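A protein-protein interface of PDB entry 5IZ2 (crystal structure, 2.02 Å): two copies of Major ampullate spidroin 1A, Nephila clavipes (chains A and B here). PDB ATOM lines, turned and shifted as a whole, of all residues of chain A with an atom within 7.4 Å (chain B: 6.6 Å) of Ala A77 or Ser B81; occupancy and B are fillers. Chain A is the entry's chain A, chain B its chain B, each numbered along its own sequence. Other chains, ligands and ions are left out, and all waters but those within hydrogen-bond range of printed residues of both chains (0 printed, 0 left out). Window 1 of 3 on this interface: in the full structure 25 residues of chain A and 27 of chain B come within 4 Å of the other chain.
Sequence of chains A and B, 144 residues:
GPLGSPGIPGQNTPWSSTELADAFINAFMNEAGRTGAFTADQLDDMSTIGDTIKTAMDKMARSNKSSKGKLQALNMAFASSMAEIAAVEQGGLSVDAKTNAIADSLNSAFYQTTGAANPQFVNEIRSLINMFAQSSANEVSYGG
Ala A77 touches just these residues of chain B: Ala B77 and Ser B81.
Ser B81 touches just these residues of chain A: Ala A73, Met A76 and Ala A77.
Of the printed residues of chain A, Glu B84 touches Gln A72 (3.2 Å) and Ala A73 (3.6 Å).
Printed residues of chain B within 4 Å of Gln A72: Glu B84 (3.2 Å).
Ala B83 touches none of the printed residues of chain A.
Asn A75 touches none of the printed residues of chain B.
The nearest printed residue of chain B that does not touch Ala A77 is Ile B49 (4.5 Å).
Ile A49 touches Leu B74, and with the chains exchanged Leu A74 touches Ile B49.
Ala A77 touches its own counterpart, Ala B77.
Ser A80 touches Ala B77, but with the chains exchanged Ala A77 does not touch Ser B80 (6.1 Å).
Leu A128 touches its own counterpart, Leu B128.
12 positions are printed for both chains.
The backbone carbonyl oxygen (O) of Ala A77 lies within hydrogen-bond range of the side-chain hydroxyl (OG) of Ser A80, 3.2 Å away.
The side-chain hydroxyl (OG) of Ser B80 lies within hydrogen-bond range of the backbone carbonyl oxygen (O) of Met B76 (2.8 Å).
OG of Ser A80 is in hydrogen-bond range of O of Met A76, at 2.6 Å.
OG of Ser A81 is in hydrogen-bond range of O of Ala A77 (2.5 Å).
O of Ala B77 lies within hydrogen-bond range of OG of Ser B81 (3.0 Å).
Of the 17 printed residues of chain B, 9 touch a printed residue of chain A.
Printed residues of chain A that touch a printed residue of chain B: Ile A49, Gln A72, Ala A73, Leu A74, Met A76, Ala A77, Ser A80, Ser A81 and Leu A128.
Among the printed residues, no Asp or Glu carboxylate lies within 4 Å of a Lys or Arg side-chain nitrogen of the other chain.
Among the printed residues, pairs that only touch across the chains: Ile A49 with Leu B74, Ala A73 with Ile B49, Ala A73 with Glu B84, Ala A73 with Ile B85, Leu A74 with Ile B49, Met A76 with Ser B81, Met A76 with Phe B132, Ala A77 with Ala B77, Ser A80 with Ala B77, Ser A80 with Ser B80, Ser A81 with Leu B74, Ser A81 with Ala B77, Leu A128 with Ser B80 and Leu A128 with Leu B128.
O of Ala A73 lies within hydrogen-bond range of OG of Ser B81 (3.3 Å).
The side-chain hydroxyl (OG) of Ser B81 lies close to the backbone NH (N) of Ala A77, 3.2 Å away.
OE2 of Glu B84 sits close to NE2 of Gln A72 (3.3 Å).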
ATOM      1  N   ILE A  49     -22.575 -21.706  32.216  1.00  0.00           N
ATOM      2  CA  ILE A  49     -21.722 -21.007  31.264  1.00  0.00           C
ATOM      3  C   ILE A  49     -21.037 -21.994  30.317  1.00  0.00           C
ATOM      4  O   ILE A  49     -20.967 -21.765  29.111  1.00  0.00           O
ATOM      5  CB  ILE A  49     -20.691 -20.138  32.000  1.00  0.00           C
ATOM      6  CG1 ILE A  49     -21.435 -19.032  32.757  1.00  0.00           C
ATOM      7  CG2 ILE A  49     -19.703 -19.528  31.013  1.00  0.00           C
ATOM      8  CD1 ILE A  49     -20.682 -18.441  33.919  1.00  0.00           C
ATOM      9  N   ILE A  53     -21.622 -22.192  26.160  1.00  0.00           N
ATOM     10  CA  ILE A  53     -20.540 -22.096  25.185  1.00  0.00           C
ATOM     11  C   ILE A  53     -20.483 -23.344  24.290  1.00  0.00           C
ATOM     12  O   ILE A  53     -20.388 -23.231  23.067  1.00  0.00           O
ATOM     13  CB  ILE A  53     -19.186 -21.852  25.897  1.00  0.00           C
ATOM     14  CG1 ILE A  53     -19.187 -20.439  26.513  1.00  0.00           C
ATOM     15  CG2 ILE A  53     -18.004 -22.013  24.928  1.00  0.00           C
ATOM     16  CD1 ILE A  53     -18.004 -20.147  27.412  1.00  0.00           C
ATOM     17  N   LEU A  71     -13.186 -20.403  18.234  1.00  0.00           N
ATOM     18  CA  LEU A  71     -12.958 -21.419  19.264  1.00  0.00           C
ATOM     19  C   LEU A  71     -11.913 -20.992  20.293  1.00  0.00           C
ATOM     20  O   LEU A  71     -12.079 -21.244  21.484  1.00  0.00           O
ATOM     21  CB  LEU A  71     -12.533 -22.757  18.637  1.00  0.00           C
ATOM     22  CG  LEU A  71     -13.586 -23.498  17.800  1.00  0.00           C
ATOM     23  CD1 LEU A  71     -13.091 -24.895  17.431  1.00  0.00           C
ATOM     24  CD2 LEU A  71     -14.930 -23.563  18.508  1.00  0.00           C
ATOM     25  N   GLN A  72     -10.841 -20.343  19.846  1.00  0.00           N
ATOM     26  CA  GLN A  72      -9.831 -19.884  20.789  1.00  0.00           C
ATOM     27  C   GLN A  72     -10.380 -18.761  21.675  1.00  0.00           C
ATOM     28  O   GLN A  72     -10.119 -18.717  22.874  1.00  0.00           O
ATOM     29  CB  GLN A  72      -8.562 -19.440  20.062  1.00  0.00           C
ATOM     30  CG  GLN A  72      -7.445 -19.108  21.024  1.00  0.00           C
ATOM     31  CD  GLN A  72      -6.117 -18.885  20.342  1.00  0.00           C
ATOM     32  OE1 GLN A  72      -6.028 -18.864  19.118  1.00  0.00           O
ATOM     33  NE2 GLN A  72      -5.069 -18.737  21.139  1.00  0.00           N
ATOM     34  N   ALA A  73     -11.149 -17.853  21.081  1.00  0.00           N
ATOM     35  CA  ALA A  73     -11.747 -16.766  21.844  1.00  0.00           C
ATOM     36  C   ALA A  73     -12.802 -17.291  22.822  1.00  0.00           C
ATOM     37  O   ALA A  73     -12.919 -16.794  23.943  1.00  0.00           O
ATOM     38  CB  ALA A  73     -12.346 -15.722  20.905  1.00  0.00           C
ATOM     39  N   LEU A  74     -13.585 -18.277  22.386  1.00  0.00           N
ATOM     40  CA  LEU A  74     -14.599 -18.881  23.250  1.00  0.00           C
ATOM     41  C   LEU A  74     -13.929 -19.648  24.386  1.00  0.00           C
ATOM     42  O   LEU A  74     -14.427 -19.668  25.508  1.00  0.00           O
ATOM     43  CB  LEU A  74     -15.526 -19.803  22.447  1.00  0.00           C
ATOM     44  CG  LEU A  74     -16.659 -19.096  21.682  1.00  0.00           C
ATOM     45  CD1 LEU A  74     -17.323 -20.044  20.700  1.00  0.00           C
ATOM     46  CD2 LEU A  74     -17.706 -18.515  22.634  1.00  0.00           C
ATOM     47  N   ASN A  75     -12.781 -20.250  24.101  1.00  0.00           N
ATOM     48  CA  ASN A  75     -12.011 -20.921  25.145  1.00  0.00           C
ATOM     49  C   ASN A  75     -11.513 -19.933  26.202  1.00  0.00           C
ATOM     50  O   ASN A  75     -11.529 -20.236  27.396  1.00  0.00           O
ATOM     51  CB  ASN A  75     -10.835 -21.682  24.534  1.00  0.00           C
ATOM     52  CG  ASN A  75      -9.932 -22.311  25.588  1.00  0.00           C
ATOM     53  OD1 ASN A  75      -9.000 -21.676  26.073  1.00  0.00           O
ATOM     54  ND2 ASN A  75     -10.214 -23.558  25.954  1.00  0.00           N
ATOM     55  N   MET A  76     -11.080 -18.749  25.768  1.00  0.00           N
ATOM     56  CA  MET A  76     -10.668 -17.714  26.713  1.00  0.00           C
ATOM     57  C   MET A  76     -11.858 -17.167  27.504  1.00  0.00           C
ATOM     58  O   MET A  76     -11.722 -16.855  28.685  1.00  0.00           O
ATOM     59  CB  MET A  76      -9.945 -16.572  25.990  1.00  0.00           C
ATOM     60  CG  MET A  76      -9.458 -15.453  26.911  1.00  0.00           C
ATOM     61  SD  MET A  76      -8.363 -16.050  28.224  1.00  0.00           S
ATOM     62  CE  MET A  76      -7.047 -16.796  27.269  1.00  0.00           C
ATOM     63  N   ALA A  77     -13.017 -17.049  26.855  1.00  0.00           N
ATOM     64  CA  ALA A  77     -14.236 -16.623  27.549  1.00  0.00           C
ATOM     65  C   ALA A  77     -14.582 -17.613  28.642  1.00  0.00           C
ATOM     66  O   ALA A  77     -14.959 -17.229  29.750  1.00  0.00           O
ATOM     67  CB  ALA A  77     -15.400 -16.500  26.582  1.00  0.00           C
ATOM     68  N   PHE A  78     -14.462 -18.894  28.312  1.00  0.00           N
ATOM     69  CA  PHE A  78     -14.709 -19.950  29.283  1.00  0.00           C
ATOM     70  C   PHE A  78     -13.718 -19.881  30.447  1.00  0.00           C
ATOM     71  O   PHE A  78     -14.125 -19.791  31.605  1.00  0.00           O
ATOM     72  CB  PHE A  78     -14.645 -21.324  28.613  1.00  0.00           C
ATOM     73  CG  PHE A  78     -14.758 -22.463  29.581  1.00  0.00           C
ATOM     74  CD1 PHE A  78     -15.971 -22.750  30.183  1.00  0.00           C
ATOM     75  CD2 PHE A  78     -13.654 -23.241  29.898  1.00  0.00           C
ATOM     76  CE1 PHE A  78     -16.086 -23.796  31.083  1.00  0.00           C
ATOM     77  CE2 PHE A  78     -13.763 -24.291  30.797  1.00  0.00           C
ATOM     78  CZ  PHE A  78     -14.975 -24.565  31.391  1.00  0.00           C
ATOM     79  N   ALA A  79     -12.421 -19.861  30.140  1.00  0.00           N
ATOM     80  CA  ALA A  79     -11.409 -19.899  31.200  1.00  0.00           C
ATOM     81  C   ALA A  79     -11.455 -18.659  32.086  1.00  0.00           C
ATOM     82  O   ALA A  79     -11.334 -18.764  33.306  1.00  0.00           O
ATOM     83  CB  ALA A  79     -10.013 -20.064  30.601  1.00  0.00           C
ATOM     84  N   SER A  80     -11.644 -17.491  31.479  1.00  0.00           N
ATOM     85  CA  SER A  80     -11.783 -16.256  32.247  1.00  0.00           C
ATOM     86  C   SER A  80     -13.086 -16.255  33.055  1.00  0.00           C
ATOM     87  O   SER A  80     -13.101 -15.785  34.190  1.00  0.00           O
ATOM     88  CB  SER A  80     -11.706 -15.021  31.337  1.00  0.00           C
ATOM     89  OG  SER A  80     -12.709 -15.052  30.336  1.00  0.00           O
ATOM     90  N   SER A  81     -14.172 -16.775  32.478  1.00  0.00           N
ATOM     91  CA  SER A  81     -15.427 -16.924  33.231  1.00  0.00           C
ATOM     92  C   SER A  81     -15.275 -17.830  34.439  1.00  0.00           C
ATOM     93  O   SER A  81     -15.710 -17.477  35.529  1.00  0.00           O
ATOM     94  CB  SER A  81     -16.554 -17.503  32.364  1.00  0.00           C
ATOM     95  OG  SER A  81     -16.903 -16.654  31.290  1.00  0.00           O
ATOM     96  N   MET A  82     -14.661 -18.997  34.248  1.00  0.00           N
ATOM     97  CA  MET A  82     -14.490 -19.940  35.352  1.00  0.00           C
ATOM     98  C   MET A  82     -13.723 -19.283  36.483  1.00  0.00           C
ATOM     99  O   MET A  82     -14.085 -19.425  37.651  1.00  0.00           O
ATOM    100  CB  MET A  82     -13.765 -21.213  34.896  1.00  0.00           C
ATOM    101  CG  MET A  82     -14.504 -22.029  33.836  1.00  0.00           C
ATOM    102  SD  MET A  82     -16.196 -22.496  34.283  1.00  0.00           S
ATOM    103  CE  MET A  82     -17.190 -21.298  33.383  1.00  0.00           C
ATOM    104  N   ALA A  83     -12.668 -18.556  36.132  1.00  0.00           N
ATOM    105  CA  ALA A  83     -11.856 -17.881  37.133  1.00  0.00           C
ATOM    106  C   ALA A  83     -12.628 -16.773  37.861  1.00  0.00           C
ATOM    107  O   ALA A  83     -12.616 -16.701  39.094  1.00  0.00           O
ATOM    108  CB  ALA A  83     -10.606 -17.309  36.486  1.00  0.00           C
ATOM    109  N   PHE A 121      -0.383 -21.299  29.445  1.00  0.00           N
ATOM    110  CA  PHE A 121      -1.773 -20.859  29.464  1.00  0.00           C
ATOM    111  C   PHE A 121      -2.238 -20.586  30.890  1.00  0.00           C
ATOM    112  O   PHE A 121      -2.855 -19.560  31.168  1.00  0.00           O
ATOM    113  CB  PHE A 121      -2.673 -21.907  28.810  1.00  0.00           C
ATOM    114  CG  PHE A 121      -4.089 -21.451  28.605  1.00  0.00           C
ATOM    115  CD1 PHE A 121      -4.475 -20.860  27.412  1.00  0.00           C
ATOM    116  CD2 PHE A 121      -5.039 -21.618  29.604  1.00  0.00           C
ATOM    117  CE1 PHE A 121      -5.784 -20.441  27.219  1.00  0.00           C
ATOM    118  CE2 PHE A 121      -6.347 -21.207  29.415  1.00  0.00           C
ATOM    119  CZ  PHE A 121      -6.719 -20.616  28.221  1.00  0.00           C
ATOM    120  N   LEU A 128      -4.367 -13.076  34.853  1.00  0.00           N
ATOM    121  CA  LEU A 128      -5.644 -12.441  34.554  1.00  0.00           C
ATOM    122  C   LEU A 128      -6.406 -12.192  35.848  1.00  0.00           C
ATOM    123  O   LEU A 128      -6.976 -11.118  36.047  1.00  0.00           O
ATOM    124  CB  LEU A 128      -6.472 -13.313  33.600  1.00  0.00           C
ATOM    125  CG  LEU A 128      -7.790 -12.764  33.043  1.00  0.00           C
ATOM    126  CD1 LEU A 128      -8.033 -13.288  31.636  1.00  0.00           C
ATOM    127  CD2 LEU A 128      -8.959 -13.144  33.942  1.00  0.00           C
ATOM    128  N   MET B  46     -15.678 -11.418  17.464  1.00  0.00           N
ATOM    129  CA  MET B  46     -16.150 -10.637  18.609  1.00  0.00           C
ATOM    130  C   MET B  46     -17.652 -10.780  18.795  1.00  0.00           C
ATOM    131  O   MET B  46     -18.137 -10.936  19.913  1.00  0.00           O
ATOM    132  CB  MET B  46     -15.815  -9.151  18.447  1.00  0.00           C
ATOM    133  CG  MET B  46     -14.327  -8.833  18.444  1.00  0.00           C
ATOM    134  SD  MET B  46     -14.080  -7.065  18.149  1.00  0.00           S
ATOM    135  CE  MET B  46     -12.288  -6.986  18.193  1.00  0.00           C
ATOM    136  N   ILE B  49     -18.572 -14.094  20.367  1.00  0.00           N
ATOM    137  CA  ILE B  49     -18.355 -14.068  21.816  1.00  0.00           C
ATOM    138  C   ILE B  49     -19.454 -13.280  22.537  1.00  0.00           C
ATOM    139  O   ILE B  49     -19.999 -13.728  23.555  1.00  0.00           O
ATOM    140  CB  ILE B  49     -17.002 -13.423  22.193  1.00  0.00           C
ATOM    141  CG1 ILE B  49     -15.827 -14.194  21.591  1.00  0.00           C
ATOM    142  CG2 ILE B  49     -16.871 -13.309  23.715  1.00  0.00           C
ATOM    143  CD1 ILE B  49     -15.786 -15.625  21.987  1.00  0.00           C
ATOM    144  N   ILE B  53     -22.065 -14.753  25.332  1.00  0.00           N
ATOM    145  CA  ILE B  53     -22.082 -14.198  26.684  1.00  0.00           C
ATOM    146  C   ILE B  53     -23.483 -13.716  27.046  1.00  0.00           C
ATOM    147  O   ILE B  53     -23.967 -13.964  28.153  1.00  0.00           O
ATOM    148  CB  ILE B  53     -21.088 -13.032  26.844  1.00  0.00           C
ATOM    149  CG1 ILE B  53     -19.644 -13.531  26.744  1.00  0.00           C
ATOM    150  CG2 ILE B  53     -21.292 -12.327  28.179  1.00  0.00           C
ATOM    151  CD1 ILE B  53     -19.242 -14.455  27.860  1.00  0.00           C
ATOM    152  N   LEU B  74     -19.211 -12.152  33.976  1.00  0.00           N
ATOM    153  CA  LEU B  74     -19.394 -12.503  32.568  1.00  0.00           C
ATOM    154  C   LEU B  74     -18.938 -11.354  31.676  1.00  0.00           C
ATOM    155  O   LEU B  74     -18.404 -11.570  30.590  1.00  0.00           O
ATOM    156  CB  LEU B  74     -20.846 -12.877  32.275  1.00  0.00           C
ATOM    157  CG  LEU B  74     -21.228 -14.312  32.661  1.00  0.00           C
ATOM    158  CD1 LEU B  74     -22.726 -14.522  32.572  1.00  0.00           C
ATOM    159  CD2 LEU B  74     -20.484 -15.328  31.797  1.00  0.00           C
ATOM    160  N   MET B  76     -16.491  -9.284  32.458  1.00  0.00           N
ATOM    161  CA  MET B  76     -15.032  -9.360  32.451  1.00  0.00           C
ATOM    162  C   MET B  76     -14.556 -10.446  31.500  1.00  0.00           C
ATOM    163  O   MET B  76     -13.550 -10.272  30.812  1.00  0.00           O
ATOM    164  CB  MET B  76     -14.490  -9.620  33.858  1.00  0.00           C
ATOM    165  CG  MET B  76     -13.956  -8.374  34.524  1.00  0.00           C
ATOM    166  SD  MET B  76     -14.716  -8.064  36.123  1.00  0.00           S
ATOM    167  CE  MET B  76     -14.273  -9.575  36.946  1.00  0.00           C
ATOM    168  N   ALA B  77     -15.277 -11.568  31.469  1.00  0.00           N
ATOM    169  CA  ALA B  77     -14.985 -12.637  30.519  1.00  0.00           C
ATOM    170  C   ALA B  77     -15.141 -12.146  29.088  1.00  0.00           C
ATOM    171  O   ALA B  77     -14.334 -12.479  28.224  1.00  0.00           O
ATOM    172  CB  ALA B  77     -15.879 -13.827  30.763  1.00  0.00           C
ATOM    173  N   PHE B  78     -16.184 -11.358  28.837  1.00  0.00           N
ATOM    174  CA  PHE B  78     -16.374 -10.778  27.510  1.00  0.00           C
ATOM    175  C   PHE B  78     -15.175  -9.918  27.120  1.00  0.00           C
ATOM    176  O   PHE B  78     -14.623 -10.057  26.031  1.00  0.00           O
ATOM    177  CB  PHE B  78     -17.651  -9.937  27.452  1.00  0.00           C
ATOM    178  CG  PHE B  78     -17.796  -9.153  26.180  1.00  0.00           C
ATOM    179  CD1 PHE B  78     -18.112  -9.786  24.989  1.00  0.00           C
ATOM    180  CD2 PHE B  78     -17.602  -7.779  26.172  1.00  0.00           C
ATOM    181  CE1 PHE B  78     -18.241  -9.060  23.809  1.00  0.00           C
ATOM    182  CE2 PHE B  78     -17.730  -7.044  24.999  1.00  0.00           C
ATOM    183  CZ  PHE B  78     -18.045  -7.685  23.819  1.00  0.00           C
ATOM    184  N   ALA B  79     -14.787  -9.014  28.009  1.00  0.00           N
ATOM    185  CA  ALA B  79     -13.695  -8.088  27.714  1.00  0.00           C
ATOM    186  C   ALA B  79     -12.361  -8.824  27.567  1.00  0.00           C
ATOM    187  O   ALA B  79     -11.522  -8.447  26.749  1.00  0.00           O
ATOM    188  CB  ALA B  79     -13.605  -7.021  28.780  1.00  0.00           C
ATOM    189  N   SER B  80     -12.167  -9.869  28.367  1.00  0.00           N
ATOM    190  CA  SER B  80     -10.953 -10.685  28.287  1.00  0.00           C
ATOM    191  C   SER B  80     -10.824 -11.391  26.934  1.00  0.00           C
ATOM    192  O   SER B  80      -9.729 -11.495  26.380  1.00  0.00           O
ATOM    193  CB  SER B  80     -10.945 -11.741  29.407  1.00  0.00           C
ATOM    194  OG  SER B  80     -10.865 -11.132  30.682  1.00  0.00           O
ATOM    195  N   SER B  81     -11.946 -11.889  26.421  1.00  0.00           N
ATOM    196  CA  SER B  81     -12.009 -12.468  25.082  1.00  0.00           C
ATOM    197  C   SER B  81     -11.682 -11.425  24.009  1.00  0.00           C
ATOM    198  O   SER B  81     -10.949 -11.714  23.062  1.00  0.00           O
ATOM    199  CB  SER B  81     -13.391 -13.066  24.826  1.00  0.00           C
ATOM    200  OG  SER B  81     -13.647 -14.098  25.749  1.00  0.00           O
ATOM    201  N   MET B  82     -12.251 -10.225  24.145  1.00  0.00           N
ATOM    202  CA  MET B  82     -11.976  -9.145  23.193  1.00  0.00           C
ATOM    203  C   MET B  82     -10.471  -8.881  23.167  1.00  0.00           C
ATOM    204  O   MET B  82      -9.879  -8.706  22.103  1.00  0.00           O
ATOM    205  CB  MET B  82     -12.736  -7.854  23.542  1.00  0.00           C
ATOM    206  CG  MET B  82     -14.268  -7.954  23.519  1.00  0.00           C
ATOM    207  SD  MET B  82     -14.961  -8.626  21.980  1.00  0.00           S
ATOM    208  CE  MET B  82     -15.305 -10.314  22.486  1.00  0.00           C
ATOM    209  N   ALA B  83      -9.864  -8.889  24.351  1.00  0.00           N
ATOM    210  CA  ALA B  83      -8.430  -8.655  24.506  1.00  0.00           C
ATOM    211  C   ALA B  83      -7.649  -9.721  23.764  1.00  0.00           C
ATOM    212  O   ALA B  83      -6.643  -9.427  23.112  1.00  0.00           O
ATOM    213  CB  ALA B  83      -8.043  -8.643  25.978  1.00  0.00           C
ATOM    214  N   GLU B  84      -8.116 -10.965  23.869  1.00  0.00           N
ATOM    215  CA  GLU B  84      -7.434 -12.092  23.244  1.00  0.00           C
ATOM    216  C   GLU B  84      -7.549 -12.031  21.724  1.00  0.00           C
ATOM    217  O   GLU B  84      -6.570 -12.270  21.022  1.00  0.00           O
ATOM    218  CB  GLU B  84      -8.017 -13.419  23.756  1.00  0.00           C
ATOM    219  CG  GLU B  84      -7.216 -14.667  23.381  1.00  0.00           C
ATOM    220  CD  GLU B  84      -7.589 -15.228  22.014  1.00  0.00           C
ATOM    221  OE1 GLU B  84      -8.701 -14.941  21.519  1.00  0.00           O
ATOM    222  OE2 GLU B  84      -6.768 -15.959  21.430  1.00  0.00           O
ATOM    223  N   ILE B  85      -8.728 -11.680  21.217  1.00  0.00           N
ATOM    224  CA  ILE B  85      -8.904 -11.503  19.778  1.00  0.00           C
ATOM    225  C   ILE B  85      -7.979 -10.408  19.224  1.00  0.00           C
ATOM    226  O   ILE B  85      -7.347 -10.579  18.179  1.00  0.00           O
ATOM    227  CB  ILE B  85     -10.368 -11.169  19.440  1.00  0.00           C
ATOM    228  CG1 ILE B  85     -11.270 -12.373  19.727  1.00  0.00           C
ATOM    229  CG2 ILE B  85     -10.508 -10.731  17.991  1.00  0.00           C
ATOM    230  CD1 ILE B  85     -12.760 -12.065  19.584  1.00  0.00           C
ATOM    231  N   ALA B  86      -7.880  -9.297  19.947  1.00  0.00           N
ATOM    232  CA  ALA B  86      -7.029  -8.180  19.542  1.00  0.00           C
ATOM    233  C   ALA B  86      -5.538  -8.526  19.573  1.00  0.00           C
ATOM    234  O   ALA B  86      -4.772  -8.074  18.726  1.00  0.00           O
ATOM    235  CB  ALA B  86      -7.299  -6.971  20.422  1.00  0.00           C
ATOM    236  N   LEU B 128      -4.060  -6.398  29.880  1.00  0.00           N
ATOM    237  CA  LEU B 128      -4.377  -7.772  29.529  1.00  0.00           C
ATOM    238  C   LEU B 128      -3.976  -8.037  28.075  1.00  0.00           C
ATOM    239  O   LEU B 128      -3.446  -9.100  27.751  1.00  0.00           O
ATOM    240  CB  LEU B 128      -5.863  -8.039  29.764  1.00  0.00           C
ATOM    241  CG  LEU B 128      -6.358  -9.475  29.670  1.00  0.00           C
ATOM    242  CD1 LEU B 128      -5.606 -10.328  30.670  1.00  0.00           C
ATOM    243  CD2 LEU B 128      -7.851  -9.524  29.956  1.00  0.00           C
ATOM    244  N   PHE B 132      -1.290 -10.786  26.768  1.00  0.00           N
ATOM    245  CA  PHE B 132      -1.601 -11.819  25.788  1.00  0.00           C
ATOM    246  C   PHE B 132      -0.661 -11.698  24.593  1.00  0.00           C
ATOM    247  O   PHE B 132      -0.259 -12.702  23.999  1.00  0.00           O
ATOM    248  CB  PHE B 132      -3.054 -11.709  25.314  1.00  0.00           C
ATOM    249  CG  PHE B 132      -4.062 -12.220  26.301  1.00  0.00           C
ATOM    250  CD1 PHE B 132      -3.742 -13.242  27.176  1.00  0.00           C
ATOM    251  CD2 PHE B 132      -5.344 -11.693  26.333  1.00  0.00           C
ATOM    252  CE1 PHE B 132      -4.675 -13.719  28.077  1.00  0.00           C
ATOM    253  CE2 PHE B 132      -6.286 -12.169  27.232  1.00  0.00           C
ATOM    254  CZ  PHE B 132      -5.949 -13.185  28.106  1.00  0.00           C
